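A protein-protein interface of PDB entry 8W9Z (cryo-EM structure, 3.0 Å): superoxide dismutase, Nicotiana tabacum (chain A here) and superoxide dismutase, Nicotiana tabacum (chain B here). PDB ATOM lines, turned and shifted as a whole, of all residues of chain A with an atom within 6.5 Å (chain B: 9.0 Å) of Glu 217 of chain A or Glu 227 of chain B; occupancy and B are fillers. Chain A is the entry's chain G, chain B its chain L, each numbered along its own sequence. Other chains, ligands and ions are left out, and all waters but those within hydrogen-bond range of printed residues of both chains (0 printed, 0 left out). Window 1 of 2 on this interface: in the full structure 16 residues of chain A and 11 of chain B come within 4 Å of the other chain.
Of chain B, only Glu 227 and His 228 come within 4 Å of Glu 217 of chain A.
Of chain A, only Glu 217 comes within 4 Å of Glu 227 of chain B.
Of the printed residues of chain B, Ser 177 of chain A touches Ser 172 (3.95 Å).
Of the printed residues of chain A, Gly 171 of chain B touches Trp 216 (3.96 Å).
Printed residues of chain B within 4 Å of Trp 216 of chain A: Gly 171.
Printed residues of chain B within 4 Å of Tyr 221 of chain A: Tyr 231 (3.9 Å).
Of the printed residues of chain A, Asn 208 of chain B touches Gly 176.
Asp 214 of chain A touches none of the printed residues of chain B.
Trp 226 of chain B touches none of the printed residues of chain A.
The nearest residue of chain A that does not touch Glu 227 of chain B is His 218 of chain A (5.1 Å).
The nearest printed residue of chain A that does not touch Gly 171 of chain B is Ser 177 of chain A (4.6 Å).
Among the printed residues, pairs that only touch across the chains: Gly 176 of chain A with Asn 208 of chain B (3.7 Å), Ser 177 of chain A with Ser 172 of chain B (3.95 Å), Trp 216 of chain A with Gly 171 of chain B (3.96 Å), Glu 217 of chain A with Glu 227 of chain B (3.3 Å), His 218 of chain A with Tyr 231 of chain B (3.6 Å), Tyr 221 of chain A with Tyr 231 of chain B (3.9 Å) and Leu 222 of chain A with Tyr 231 of chain B (3.8 Å).
The backbone NH of His 228 of chain B sits at hydrogen-bond distance from the side-chain carboxylate of Glu 217 of chain A.
Printed residues of chain B that touch a printed residue of chain A: Gly 171, Ser 172, Asn 208, Glu 227, His 228 and Tyr 231.
Hydrophobic or aromatic side chains of chain B within 4 Å of the printed part of chain A: His 228 and Tyr 231.
N of Asn 208 of chain B is in hydrogen-bond range of O of Ser 172 of chain B, 3.0 Å away.
The side-chain carboxylate (OD1) of Asp 214 of chain A lies within hydrogen-bond range of the backbone NH (N) of Trp 216 of chain A (3.1 Å).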
ATOM      1  N   GLY A 176      -5.143  18.493 -33.365  1.00  0.00           N
ATOM      2  CA  GLY A 176      -6.149  19.504 -33.160  1.00  0.00           C
ATOM      3  C   GLY A 176      -7.223  19.387 -34.200  1.00  0.00           C
ATOM      4  O   GLY A 176      -7.349  18.355 -34.843  1.00  0.00           O
ATOM      5  N   SER A 177      -8.020  20.431 -34.353  1.00  0.00           N
ATOM      6  CA  SER A 177      -9.080  20.418 -35.331  1.00  0.00           C
ATOM      7  C   SER A 177      -8.534  20.794 -36.685  1.00  0.00           C
ATOM      8  O   SER A 177      -7.503  21.445 -36.771  1.00  0.00           O
ATOM      9  CB  SER A 177     -10.120  21.420 -34.909  1.00  0.00           C
ATOM     10  OG  SER A 177     -10.557  21.154 -33.591  1.00  0.00           O
ATOM     11  N   GLY A 178      -9.207  20.382 -37.749  1.00  0.00           N
ATOM     12  CA  GLY A 178      -8.729  20.673 -39.085  1.00  0.00           C
ATOM     13  C   GLY A 178      -9.445  19.844 -40.111  1.00  0.00           C
ATOM     14  O   GLY A 178     -10.413  19.186 -39.780  1.00  0.00           O
ATOM     15  N   ASP A 214     -13.860  15.977 -42.104  1.00  0.00           N
ATOM     16  CA  ASP A 214     -13.837  16.932 -41.009  1.00  0.00           C
ATOM     17  C   ASP A 214     -13.204  16.258 -39.844  1.00  0.00           C
ATOM     18  O   ASP A 214     -13.746  15.314 -39.302  1.00  0.00           O
ATOM     19  CB  ASP A 214     -15.258  17.322 -40.623  1.00  0.00           C
ATOM     20  CG  ASP A 214     -15.312  18.549 -39.754  1.00  0.00           C
ATOM     21  OD1 ASP A 214     -14.242  19.074 -39.414  1.00  0.00           O
ATOM     22  OD2 ASP A 214     -16.425  19.004 -39.422  1.00  0.00           O
ATOM     23  N   LEU A 215     -12.052  16.746 -39.442  1.00  0.00           N
ATOM     24  CA  LEU A 215     -11.360  16.140 -38.348  1.00  0.00           C
ATOM     25  C   LEU A 215     -11.658  16.886 -37.088  1.00  0.00           C
ATOM     26  O   LEU A 215     -11.153  16.544 -36.033  1.00  0.00           O
ATOM     27  CB  LEU A 215      -9.877  16.090 -38.624  1.00  0.00           C
ATOM     28  CG  LEU A 215      -9.512  15.100 -39.726  1.00  0.00           C
ATOM     29  CD1 LEU A 215      -8.015  15.103 -39.969  1.00  0.00           C
ATOM     30  CD2 LEU A 215      -9.988  13.710 -39.347  1.00  0.00           C
ATOM     31  N   TRP A 216     -12.488  17.906 -37.178  1.00  0.00           N
ATOM     32  CA  TRP A 216     -12.885  18.605 -35.978  1.00  0.00           C
ATOM     33  C   TRP A 216     -13.635  17.609 -35.148  1.00  0.00           C
ATOM     34  O   TRP A 216     -14.389  16.804 -35.669  1.00  0.00           O
ATOM     35  CB  TRP A 216     -13.812  19.762 -36.291  1.00  0.00           C
ATOM     36  CG  TRP A 216     -13.162  20.982 -36.798  1.00  0.00           C
ATOM     37  CD1 TRP A 216     -12.341  21.087 -37.870  1.00  0.00           C
ATOM     38  CD2 TRP A 216     -13.305  22.300 -36.272  1.00  0.00           C
ATOM     39  NE1 TRP A 216     -11.944  22.383 -38.036  1.00  0.00           N
ATOM     40  CE2 TRP A 216     -12.528  23.150 -37.066  1.00  0.00           C
ATOM     41  CE3 TRP A 216     -14.007  22.838 -35.194  1.00  0.00           C
ATOM     42  CZ2 TRP A 216     -12.433  24.510 -36.822  1.00  0.00           C
ATOM     43  CZ3 TRP A 216     -13.914  24.186 -34.955  1.00  0.00           C
ATOM     44  CH2 TRP A 216     -13.133  25.007 -35.762  1.00  0.00           C
ATOM     45  N   GLU A 217     -13.471  17.675 -33.845  1.00  0.00           N
ATOM     46  CA  GLU A 217     -14.094  16.701 -32.975  1.00  0.00           C
ATOM     47  C   GLU A 217     -15.588  16.729 -32.991  1.00  0.00           C
ATOM     48  O   GLU A 217     -16.214  15.724 -32.706  1.00  0.00           O
ATOM     49  CB  GLU A 217     -13.600  16.867 -31.552  1.00  0.00           C
ATOM     50  CG  GLU A 217     -12.106  16.647 -31.394  1.00  0.00           C
ATOM     51  CD  GLU A 217     -11.637  16.824 -29.963  1.00  0.00           C
ATOM     52  OE1 GLU A 217     -12.408  17.372 -29.151  1.00  0.00           O
ATOM     53  OE2 GLU A 217     -10.498  16.422 -29.653  1.00  0.00           O
ATOM     54  N   HIS A 218     -16.182  17.854 -33.344  1.00  0.00           N
ATOM     55  CA  HIS A 218     -17.622  17.935 -33.250  1.00  0.00           C
ATOM     56  C   HIS A 218     -18.211  16.854 -34.097  1.00  0.00           C
ATOM     57  O   HIS A 218     -19.265  16.320 -33.793  1.00  0.00           O
ATOM     58  CB  HIS A 218     -18.194  19.316 -33.596  1.00  0.00           C
ATOM     59  CG  HIS A 218     -17.741  19.889 -34.902  1.00  0.00           C
ATOM     60  ND1 HIS A 218     -17.203  21.153 -35.001  1.00  0.00           N
ATOM     61  CD2 HIS A 218     -17.792  19.405 -36.164  1.00  0.00           C
ATOM     62  CE1 HIS A 218     -16.923  21.414 -36.266  1.00  0.00           C
ATOM     63  NE2 HIS A 218     -17.266  20.367 -36.992  1.00  0.00           N
ATOM     64  N   ALA A 219     -17.541  16.540 -35.181  1.00  0.00           N
ATOM     65  CA  ALA A 219     -18.031  15.509 -36.053  1.00  0.00           C
ATOM     66  C   ALA A 219     -18.097  14.128 -35.455  1.00  0.00           C
ATOM     67  O   ALA A 219     -19.082  13.436 -35.650  1.00  0.00           O
ATOM     68  CB  ALA A 219     -17.179  15.460 -37.297  1.00  0.00           C
ATOM     69  N   TYR A 220     -17.072  13.698 -34.736  1.00  0.00           N
ATOM     70  CA  TYR A 220     -17.087  12.316 -34.271  1.00  0.00           C
ATOM     71  C   TYR A 220     -17.405  12.026 -32.820  1.00  0.00           C
ATOM     72  O   TYR A 220     -17.670  10.883 -32.479  1.00  0.00           O
ATOM     73  CB  TYR A 220     -15.798  11.598 -34.672  1.00  0.00           C
ATOM     74  CG  TYR A 220     -14.511  12.256 -34.264  1.00  0.00           C
ATOM     75  CD1 TYR A 220     -13.957  12.026 -33.018  1.00  0.00           C
ATOM     76  CD2 TYR A 220     -13.827  13.076 -35.142  1.00  0.00           C
ATOM     77  CE1 TYR A 220     -12.769  12.617 -32.647  1.00  0.00           C
ATOM     78  CE2 TYR A 220     -12.639  13.671 -34.780  1.00  0.00           C
ATOM     79  CZ  TYR A 220     -12.115  13.437 -33.532  1.00  0.00           C
ATOM     80  OH  TYR A 220     -10.930  14.029 -33.172  1.00  0.00           O
ATOM     81  N   TYR A 221     -17.454  13.032 -31.966  1.00  0.00           N
ATOM     82  CA  TYR A 221     -17.619  12.762 -30.539  1.00  0.00           C
ATOM     83  C   TYR A 221     -18.802  11.940 -30.095  1.00  0.00           C
ATOM     84  O   TYR A 221     -18.692  11.234 -29.104  1.00  0.00           O
ATOM     85  CB  TYR A 221     -17.555  14.038 -29.714  1.00  0.00           C
ATOM     86  N   LEU A 222     -19.930  12.002 -30.779  1.00  0.00           N
ATOM     87  CA  LEU A 222     -21.083  11.283 -30.263  1.00  0.00           C
ATOM     88  C   LEU A 222     -21.120   9.755 -30.428  1.00  0.00           C
ATOM     89  O   LEU A 222     -21.518   9.060 -29.504  1.00  0.00           O
ATOM     90  CB  LEU A 222     -22.366  11.927 -30.751  1.00  0.00           C
ATOM     91  CG  LEU A 222     -22.534  13.372 -30.290  1.00  0.00           C
ATOM     92  CD1 LEU A 222     -23.837  13.948 -30.812  1.00  0.00           C
ATOM     93  CD2 LEU A 222     -22.487  13.448 -28.773  1.00  0.00           C
ATOM     94  N   ASN A 226     -13.538   8.554 -28.687  1.00  0.00           N
ATOM     95  CA  ASN A 226     -12.135   8.913 -28.824  1.00  0.00           C
ATOM     96  C   ASN A 226     -11.365   8.034 -29.799  1.00  0.00           C
ATOM     97  O   ASN A 226     -10.150   8.210 -29.934  1.00  0.00           O
ATOM     98  CB  ASN A 226     -11.439   8.881 -27.455  1.00  0.00           C
ATOM     99  CG  ASN A 226     -12.055   9.855 -26.471  1.00  0.00           C
ATOM    100  OD1 ASN A 226     -12.239   9.539 -25.296  1.00  0.00           O
ATOM    101  ND2 ASN A 226     -12.390  11.045 -26.952  1.00  0.00           N
ATOM    102  N   THR B  69     -17.755  12.434 -18.398  1.00  0.00           N
ATOM    103  CA  THR B  69     -16.946  13.461 -19.007  1.00  0.00           C
ATOM    104  C   THR B  69     -15.566  13.346 -18.426  1.00  0.00           C
ATOM    105  O   THR B  69     -14.577  13.385 -19.145  1.00  0.00           O
ATOM    106  CB  THR B  69     -17.507  14.854 -18.715  1.00  0.00           C
ATOM    107  N   HIS B  73     -12.239  12.546 -20.605  1.00  0.00           N
ATOM    108  CA  HIS B  73     -11.297  13.655 -20.703  1.00  0.00           C
ATOM    109  C   HIS B  73     -10.004  13.346 -20.014  1.00  0.00           C
ATOM    110  O   HIS B  73      -8.931  13.583 -20.552  1.00  0.00           O
ATOM    111  CB  HIS B  73     -11.924  14.888 -20.065  1.00  0.00           C
ATOM    112  CG  HIS B  73     -11.170  16.156 -20.300  1.00  0.00           C
ATOM    113  ND1 HIS B  73     -11.527  17.345 -19.703  1.00  0.00           N
ATOM    114  CD2 HIS B  73     -10.089  16.428 -21.065  1.00  0.00           C
ATOM    115  CE1 HIS B  73     -10.696  18.294 -20.088  1.00  0.00           C
ATOM    116  NE2 HIS B  73      -9.814  17.765 -20.913  1.00  0.00           N
ATOM    117  N   HIS B  77      -8.189  10.653 -22.576  1.00  0.00           N
ATOM    118  CA  HIS B  77      -7.362  11.628 -23.259  1.00  0.00           C
ATOM    119  C   HIS B  77      -6.075  12.011 -22.531  1.00  0.00           C
ATOM    120  O   HIS B  77      -5.003  12.014 -23.128  1.00  0.00           O
ATOM    121  CB  HIS B  77      -8.185  12.869 -23.593  1.00  0.00           C
ATOM    122  N   TYR B  81      -2.078  11.220 -23.579  1.00  0.00           N
ATOM    123  CA  TYR B  81      -1.003  12.164 -23.798  1.00  0.00           C
ATOM    124  C   TYR B  81       0.215  11.745 -23.016  1.00  0.00           C
ATOM    125  O   TYR B  81       1.323  11.727 -23.546  1.00  0.00           O
ATOM    126  CB  TYR B  81      -1.400  13.567 -23.371  1.00  0.00           C
ATOM    127  CG  TYR B  81      -2.521  14.155 -24.172  1.00  0.00           C
ATOM    128  CD1 TYR B  81      -2.494  14.127 -25.557  1.00  0.00           C
ATOM    129  CD2 TYR B  81      -3.597  14.757 -23.547  1.00  0.00           C
ATOM    130  CE1 TYR B  81      -3.523  14.667 -26.298  1.00  0.00           C
ATOM    131  CE2 TYR B  81      -4.630  15.296 -24.280  1.00  0.00           C
ATOM    132  CZ  TYR B  81      -4.585  15.252 -25.653  1.00  0.00           C
ATOM    133  OH  TYR B  81      -5.614  15.795 -26.379  1.00  0.00           O
ATOM    134  N   HIS B 125      -3.343  19.677 -18.973  1.00  0.00           N
ATOM    135  CA  HIS B 125      -4.498  18.942 -18.532  1.00  0.00           C
ATOM    136  C   HIS B 125      -4.509  18.856 -17.036  1.00  0.00           C
ATOM    137  O   HIS B 125      -5.543  19.045 -16.414  1.00  0.00           O
ATOM    138  CB  HIS B 125      -4.529  17.554 -19.148  1.00  0.00           C
ATOM    139  CG  HIS B 125      -5.395  17.462 -20.363  1.00  0.00           C
ATOM    140  ND1 HIS B 125      -4.997  17.922 -21.598  1.00  0.00           N
ATOM    141  CD2 HIS B 125      -6.648  16.978 -20.530  1.00  0.00           C
ATOM    142  CE1 HIS B 125      -5.968  17.731 -22.472  1.00  0.00           C
ATOM    143  NE2 HIS B 125      -6.977  17.151 -21.851  1.00  0.00           N
ATOM    144  N   GLN B 169     -12.189  31.903 -28.645  1.00  0.00           N
ATOM    145  CA  GLN B 169     -11.169  31.014 -29.152  1.00  0.00           C
ATOM    146  C   GLN B 169     -11.799  30.190 -30.236  1.00  0.00           C
ATOM    147  O   GLN B 169     -12.908  29.690 -30.075  1.00  0.00           O
ATOM    148  CB  GLN B 169     -10.585  30.129 -28.062  1.00  0.00           C
ATOM    149  CG  GLN B 169      -9.611  29.073 -28.552  1.00  0.00           C
ATOM    150  CD  GLN B 169      -8.337  29.658 -29.117  1.00  0.00           C
ATOM    151  OE1 GLN B 169      -7.967  30.789 -28.810  1.00  0.00           O
ATOM    152  NE2 GLN B 169      -7.648  28.880 -29.937  1.00  0.00           N
ATOM    153  N   GLY B 171     -11.488  26.878 -32.557  1.00  0.00           N
ATOM    154  CA  GLY B 171     -10.794  25.616 -32.627  1.00  0.00           C
ATOM    155  C   GLY B 171     -10.348  25.159 -31.265  1.00  0.00           C
ATOM    156  O   GLY B 171     -10.778  25.700 -30.256  1.00  0.00           O
ATOM    157  N   SER B 172      -9.506  24.143 -31.226  1.00  0.00           N
ATOM    158  CA  SER B 172      -9.007  23.662 -29.966  1.00  0.00           C
ATOM    159  C   SER B 172      -8.101  24.688 -29.326  1.00  0.00           C
ATOM    160  O   SER B 172      -7.307  25.327 -30.004  1.00  0.00           O
ATOM    161  CB  SER B 172      -8.256  22.366 -30.180  1.00  0.00           C
ATOM    162  OG  SER B 172      -7.670  21.908 -28.971  1.00  0.00           O
ATOM    163  N   GLY B 173      -8.233  24.864 -28.016  1.00  0.00           N
ATOM    164  CA  GLY B 173      -7.427  25.842 -27.322  1.00  0.00           C
ATOM    165  C   GLY B 173      -7.561  25.808 -25.824  1.00  0.00           C
ATOM    166  O   GLY B 173      -8.320  25.004 -25.295  1.00  0.00           O
ATOM    167  N   TRP B 174      -6.824  26.669 -25.134  1.00  0.00           N
ATOM    168  CA  TRP B 174      -6.945  26.770 -23.692  1.00  0.00           C
ATOM    169  C   TRP B 174      -7.060  28.243 -23.387  1.00  0.00           C
ATOM    170  O   TRP B 174      -6.697  29.075 -24.207  1.00  0.00           O
ATOM    171  CB  TRP B 174      -5.712  26.222 -22.993  1.00  0.00           C
ATOM    172  CG  TRP B 174      -5.391  24.807 -23.265  1.00  0.00           C
ATOM    173  CD1 TRP B 174      -4.748  24.307 -24.354  1.00  0.00           C
ATOM    174  CD2 TRP B 174      -5.660  23.697 -22.412  1.00  0.00           C
ATOM    175  NE1 TRP B 174      -4.618  22.949 -24.241  1.00  0.00           N
ATOM    176  CE2 TRP B 174      -5.170  22.550 -23.056  1.00  0.00           C
ATOM    177  CE3 TRP B 174      -6.278  23.560 -21.170  1.00  0.00           C
ATOM    178  CZ2 TRP B 174      -5.278  21.284 -22.500  1.00  0.00           C
ATOM    179  CZ3 TRP B 174      -6.378  22.309 -20.618  1.00  0.00           C
ATOM    180  CH2 TRP B 174      -5.882  21.186 -21.281  1.00  0.00           C
ATOM    181  N   ASN B 208      -4.260  25.343 -29.913  1.00  0.00           N
ATOM    182  CA  ASN B 208      -4.169  24.026 -29.333  1.00  0.00           C
ATOM    183  C   ASN B 208      -2.774  23.690 -28.880  1.00  0.00           C
ATOM    184  O   ASN B 208      -1.819  23.896 -29.615  1.00  0.00           O
ATOM    185  CB  ASN B 208      -4.605  22.985 -30.349  1.00  0.00           C
ATOM    186  CG  ASN B 208      -4.264  23.365 -31.783  1.00  0.00           C
ATOM    187  OD1 ASN B 208      -3.229  23.967 -32.060  1.00  0.00           O
ATOM    188  ND2 ASN B 208      -5.136  22.986 -32.707  1.00  0.00           N
ATOM    189  N   ASP B 224     -10.220  24.169 -20.459  1.00  0.00           N
ATOM    190  CA  ASP B 224      -9.940  23.393 -21.645  1.00  0.00           C
ATOM    191  C   ASP B 224     -11.066  23.678 -22.575  1.00  0.00           C
ATOM    192  O   ASP B 224     -12.165  23.183 -22.382  1.00  0.00           O
ATOM    193  CB  ASP B 224      -9.911  21.905 -21.367  1.00  0.00           C
ATOM    194  CG  ASP B 224      -9.075  21.150 -22.376  1.00  0.00           C
ATOM    195  OD1 ASP B 224      -8.678  21.752 -23.390  1.00  0.00           O
ATOM    196  OD2 ASP B 224      -8.773  19.967 -22.148  1.00  0.00           O
ATOM    197  N   VAL B 225     -10.814  24.501 -23.593  1.00  0.00           N
ATOM    198  CA  VAL B 225     -11.862  24.855 -24.536  1.00  0.00           C
ATOM    199  C   VAL B 225     -11.827  23.873 -25.667  1.00  0.00           C
ATOM    200  O   VAL B 225     -12.682  23.898 -26.540  1.00  0.00           O
ATOM    201  CB  VAL B 225     -11.795  26.309 -25.019  1.00  0.00           C
ATOM    202  CG1 VAL B 225     -11.344  27.225 -23.897  1.00  0.00           C
ATOM    203  CG2 VAL B 225     -10.892  26.463 -26.225  1.00  0.00           C
ATOM    204  N   TRP B 226     -10.887  22.944 -25.627  1.00  0.00           N
ATOM    205  CA  TRP B 226     -10.891  21.929 -26.641  1.00  0.00           C
ATOM    206  C   TRP B 226     -12.204  21.207 -26.453  1.00  0.00           C
ATOM    207  O   TRP B 226     -12.680  21.057 -25.336  1.00  0.00           O
ATOM    208  CB  TRP B 226      -9.678  21.017 -26.545  1.00  0.00           C
ATOM    209  N   GLU B 227     -12.799  20.742 -27.533  1.00  0.00           N
ATOM    210  CA  GLU B 227     -14.135  20.152 -27.468  1.00  0.00           C
ATOM    211  C   GLU B 227     -14.325  18.925 -26.643  1.00  0.00           C
ATOM    212  O   GLU B 227     -15.437  18.661 -26.201  1.00  0.00           O
ATOM    213  CB  GLU B 227     -14.621  19.829 -28.869  1.00  0.00           C
ATOM    214  N   HIS B 228     -13.274  18.157 -26.422  1.00  0.00           N
ATOM    215  CA  HIS B 228     -13.465  16.911 -25.722  1.00  0.00           C
ATOM    216  C   HIS B 228     -14.075  17.259 -24.403  1.00  0.00           C
ATOM    217  O   HIS B 228     -14.916  16.534 -23.895  1.00  0.00           O
ATOM    218  CB  HIS B 228     -12.169  16.105 -25.569  1.00  0.00           C
ATOM    219  CG  HIS B 228     -10.974  16.904 -25.154  1.00  0.00           C
ATOM    220  ND1 HIS B 228      -9.846  17.005 -25.938  1.00  0.00           N
ATOM    221  CD2 HIS B 228     -10.707  17.597 -24.024  1.00  0.00           C
ATOM    222  CE1 HIS B 228      -8.944  17.742 -25.316  1.00  0.00           C
ATOM    223  NE2 HIS B 228      -9.441  18.115 -24.153  1.00  0.00           N
ATOM    224  N   ALA B 229     -13.682  18.382 -23.853  1.00  0.00           N
ATOM    225  CA  ALA B 229     -14.164  18.749 -22.555  1.00  0.00           C
ATOM    226  C   ALA B 229     -15.641  18.978 -22.354  1.00  0.00           C
ATOM    227  O   ALA B 229     -16.193  18.488 -21.388  1.00  0.00           O
ATOM    228  CB  ALA B 229     -13.433  19.991 -22.116  1.00  0.00           C
ATOM    229  N   TYR B 230     -16.311  19.698 -23.231  1.00  0.00           N
ATOM    230  CA  TYR B 230     -17.707  20.032 -22.938  1.00  0.00           C
ATOM    231  C   TYR B 230     -18.774  19.484 -23.816  1.00  0.00           C
ATOM    232  O   TYR B 230     -19.951  19.659 -23.532  1.00  0.00           O
ATOM    233  CB  TYR B 230     -17.878  21.537 -22.943  1.00  0.00           C
ATOM    234  CG  TYR B 230     -17.429  22.223 -24.211  1.00  0.00           C
ATOM    235  CD1 TYR B 230     -16.114  22.626 -24.369  1.00  0.00           C
ATOM    236  CD2 TYR B 230     -18.321  22.490 -25.235  1.00  0.00           C
ATOM    237  CE1 TYR B 230     -15.697  23.259 -25.517  1.00  0.00           C
ATOM    238  CE2 TYR B 230     -17.910  23.121 -26.388  1.00  0.00           C
ATOM    239  CZ  TYR B 230     -16.595  23.504 -26.519  1.00  0.00           C
ATOM    240  OH  TYR B 230     -16.171  24.139 -27.659  1.00  0.00           O
ATOM    241  N   TYR B 231     -18.394  18.819 -24.883  1.00  0.00           N
ATOM    242  CA  TYR B 231     -19.393  18.392 -25.835  1.00  0.00           C
ATOM    243  C   TYR B 231     -20.367  17.451 -25.220  1.00  0.00           C
ATOM    244  O   TYR B 231     -21.556  17.702 -25.221  1.00  0.00           O
ATOM    245  CB  TYR B 231     -18.731  17.717 -27.022  1.00  0.00           C
ATOM    246  CG  TYR B 231     -19.530  17.815 -28.285  1.00  0.00           C
ATOM    247  CD1 TYR B 231     -19.591  19.003 -28.989  1.00  0.00           C
ATOM    248  CD2 TYR B 231     -20.221  16.724 -28.777  1.00  0.00           C
ATOM    249  CE1 TYR B 231     -20.321  19.102 -30.151  1.00  0.00           C
ATOM    250  CE2 TYR B 231     -20.954  16.813 -29.940  1.00  0.00           C
ATOM    251  CZ  TYR B 231     -21.000  18.006 -30.620  1.00  0.00           C
ATOM    252  OH  TYR B 231     -21.725  18.104 -31.781  1.00  0.00           O
ATOM    253  N   LEU B 232     -19.870  16.354 -24.698  1.00  0.00           N
ATOM    254  CA  LEU B 232     -20.741  15.347 -24.167  1.00  0.00           C
ATOM    255  C   LEU B 232     -21.745  15.998 -23.249  1.00  0.00           C
ATOM    256  O   LEU B 232     -22.934  15.711 -23.313  1.00  0.00           O
ATOM    257  CB  LEU B 232     -19.934  14.307 -23.415  1.00  0.00           C
ATOM    258  CG  LEU B 232     -18.844  13.623 -24.238  1.00  0.00           C
ATOM    259  CD1 LEU B 232     -17.935  12.794 -23.347  1.00  0.00           C
ATOM    260  CD2 LEU B 232     -19.450  12.770 -25.341  1.00  0.00           C
ATOM    261  N   ASP B 233     -21.266  16.875 -22.385  1.00  0.00           N
ATOM    262  CA  ASP B 233     -22.159  17.542 -21.451  1.00  0.00           C
ATOM    263  C   ASP B 233     -23.119  18.574 -21.999  1.00  0.00           C
ATOM    264  O   ASP B 233     -24.300  18.554 -21.676  1.00  0.00           O
ATOM    265  CB  ASP B 233     -21.336  18.201 -20.351  1.00  0.00           C
ATOM    266  N   PHE B 234     -22.629  19.470 -22.840  1.00  0.00           N
ATOM    267  CA  PHE B 234     -23.472  20.563 -23.307  1.00  0.00           C
ATOM    268  C   PHE B 234     -23.749  20.584 -24.797  1.00  0.00           C
ATOM    269  O   PHE B 234     -24.377  21.522 -25.282  1.00  0.00           O
ATOM    270  CB  PHE B 234     -22.882  21.897 -22.849  1.00  0.00           C
ATOM    271  N   ARG B 235     -23.265  19.591 -25.531  1.00  0.00           N
ATOM    272  CA  ARG B 235     -23.588  19.497 -26.953  1.00  0.00           C
ATOM    273  C   ARG B 235     -23.321  20.770 -27.705  1.00  0.00           C
ATOM    274  O   ARG B 235     -24.232  21.274 -28.354  1.00  0.00           O
ATOM    275  CB  ARG B 235     -25.031  19.042 -27.162  1.00  0.00           C
ATOM    276  N   ASN B 236     -22.135  21.338 -27.547  1.00  0.00           N
ATOM    277  CA  ASN B 236     -21.736  22.538 -28.291  1.00  0.00           C
ATOM    278  C   ASN B 236     -22.251  23.864 -27.795  1.00  0.00           C
ATOM    279  O   ASN B 236     -22.075  24.875 -28.466  1.00  0.00           O
ATOM    280  CB  ASN B 236     -22.001  22.420 -29.789  1.00  0.00           C
ATOM    281  N   ARG B 238     -21.034  26.080 -25.980  1.00  0.00           N
ATOM    282  CA  ARG B 238     -19.804  26.456 -25.290  1.00  0.00           C
ATOM    283  C   ARG B 238     -19.926  27.595 -24.315  1.00  0.00           C
ATOM    284  O   ARG B 238     -19.302  27.568 -23.268  1.00  0.00           O
ATOM    285  CB  ARG B 238     -18.657  26.723 -26.264  1.00  0.00           C
ATOM    286  N   TYR B 241     -20.852  26.193 -20.803  1.00  0.00           N
ATOM    287  CA  TYR B 241     -19.774  25.520 -20.115  1.00  0.00           C
ATOM    288  C   TYR B 241     -18.865  26.545 -19.497  1.00  0.00           C
ATOM    289  O   TYR B 241     -18.512  26.432 -18.334  1.00  0.00           O
ATOM    290  CB  TYR B 241     -19.029  24.639 -21.102  1.00  0.00           C
ATOM    291  CG  TYR B 241     -17.605  24.263 -20.781  1.00  0.00           C
ATOM    292  CD1 TYR B 241     -17.316  23.277 -19.855  1.00  0.00           C
ATOM    293  CD2 TYR B 241     -16.550  24.846 -21.463  1.00  0.00           C
ATOM    294  CE1 TYR B 241     -16.014  22.915 -19.586  1.00  0.00           C
ATOM    295  CE2 TYR B 241     -15.246  24.493 -21.199  1.00  0.00           C
ATOM    296  CZ  TYR B 241     -14.983  23.525 -20.260  1.00  0.00           C
ATOM    297  OH  TYR B 241     -13.682  23.172 -19.997  1.00  0.00           O
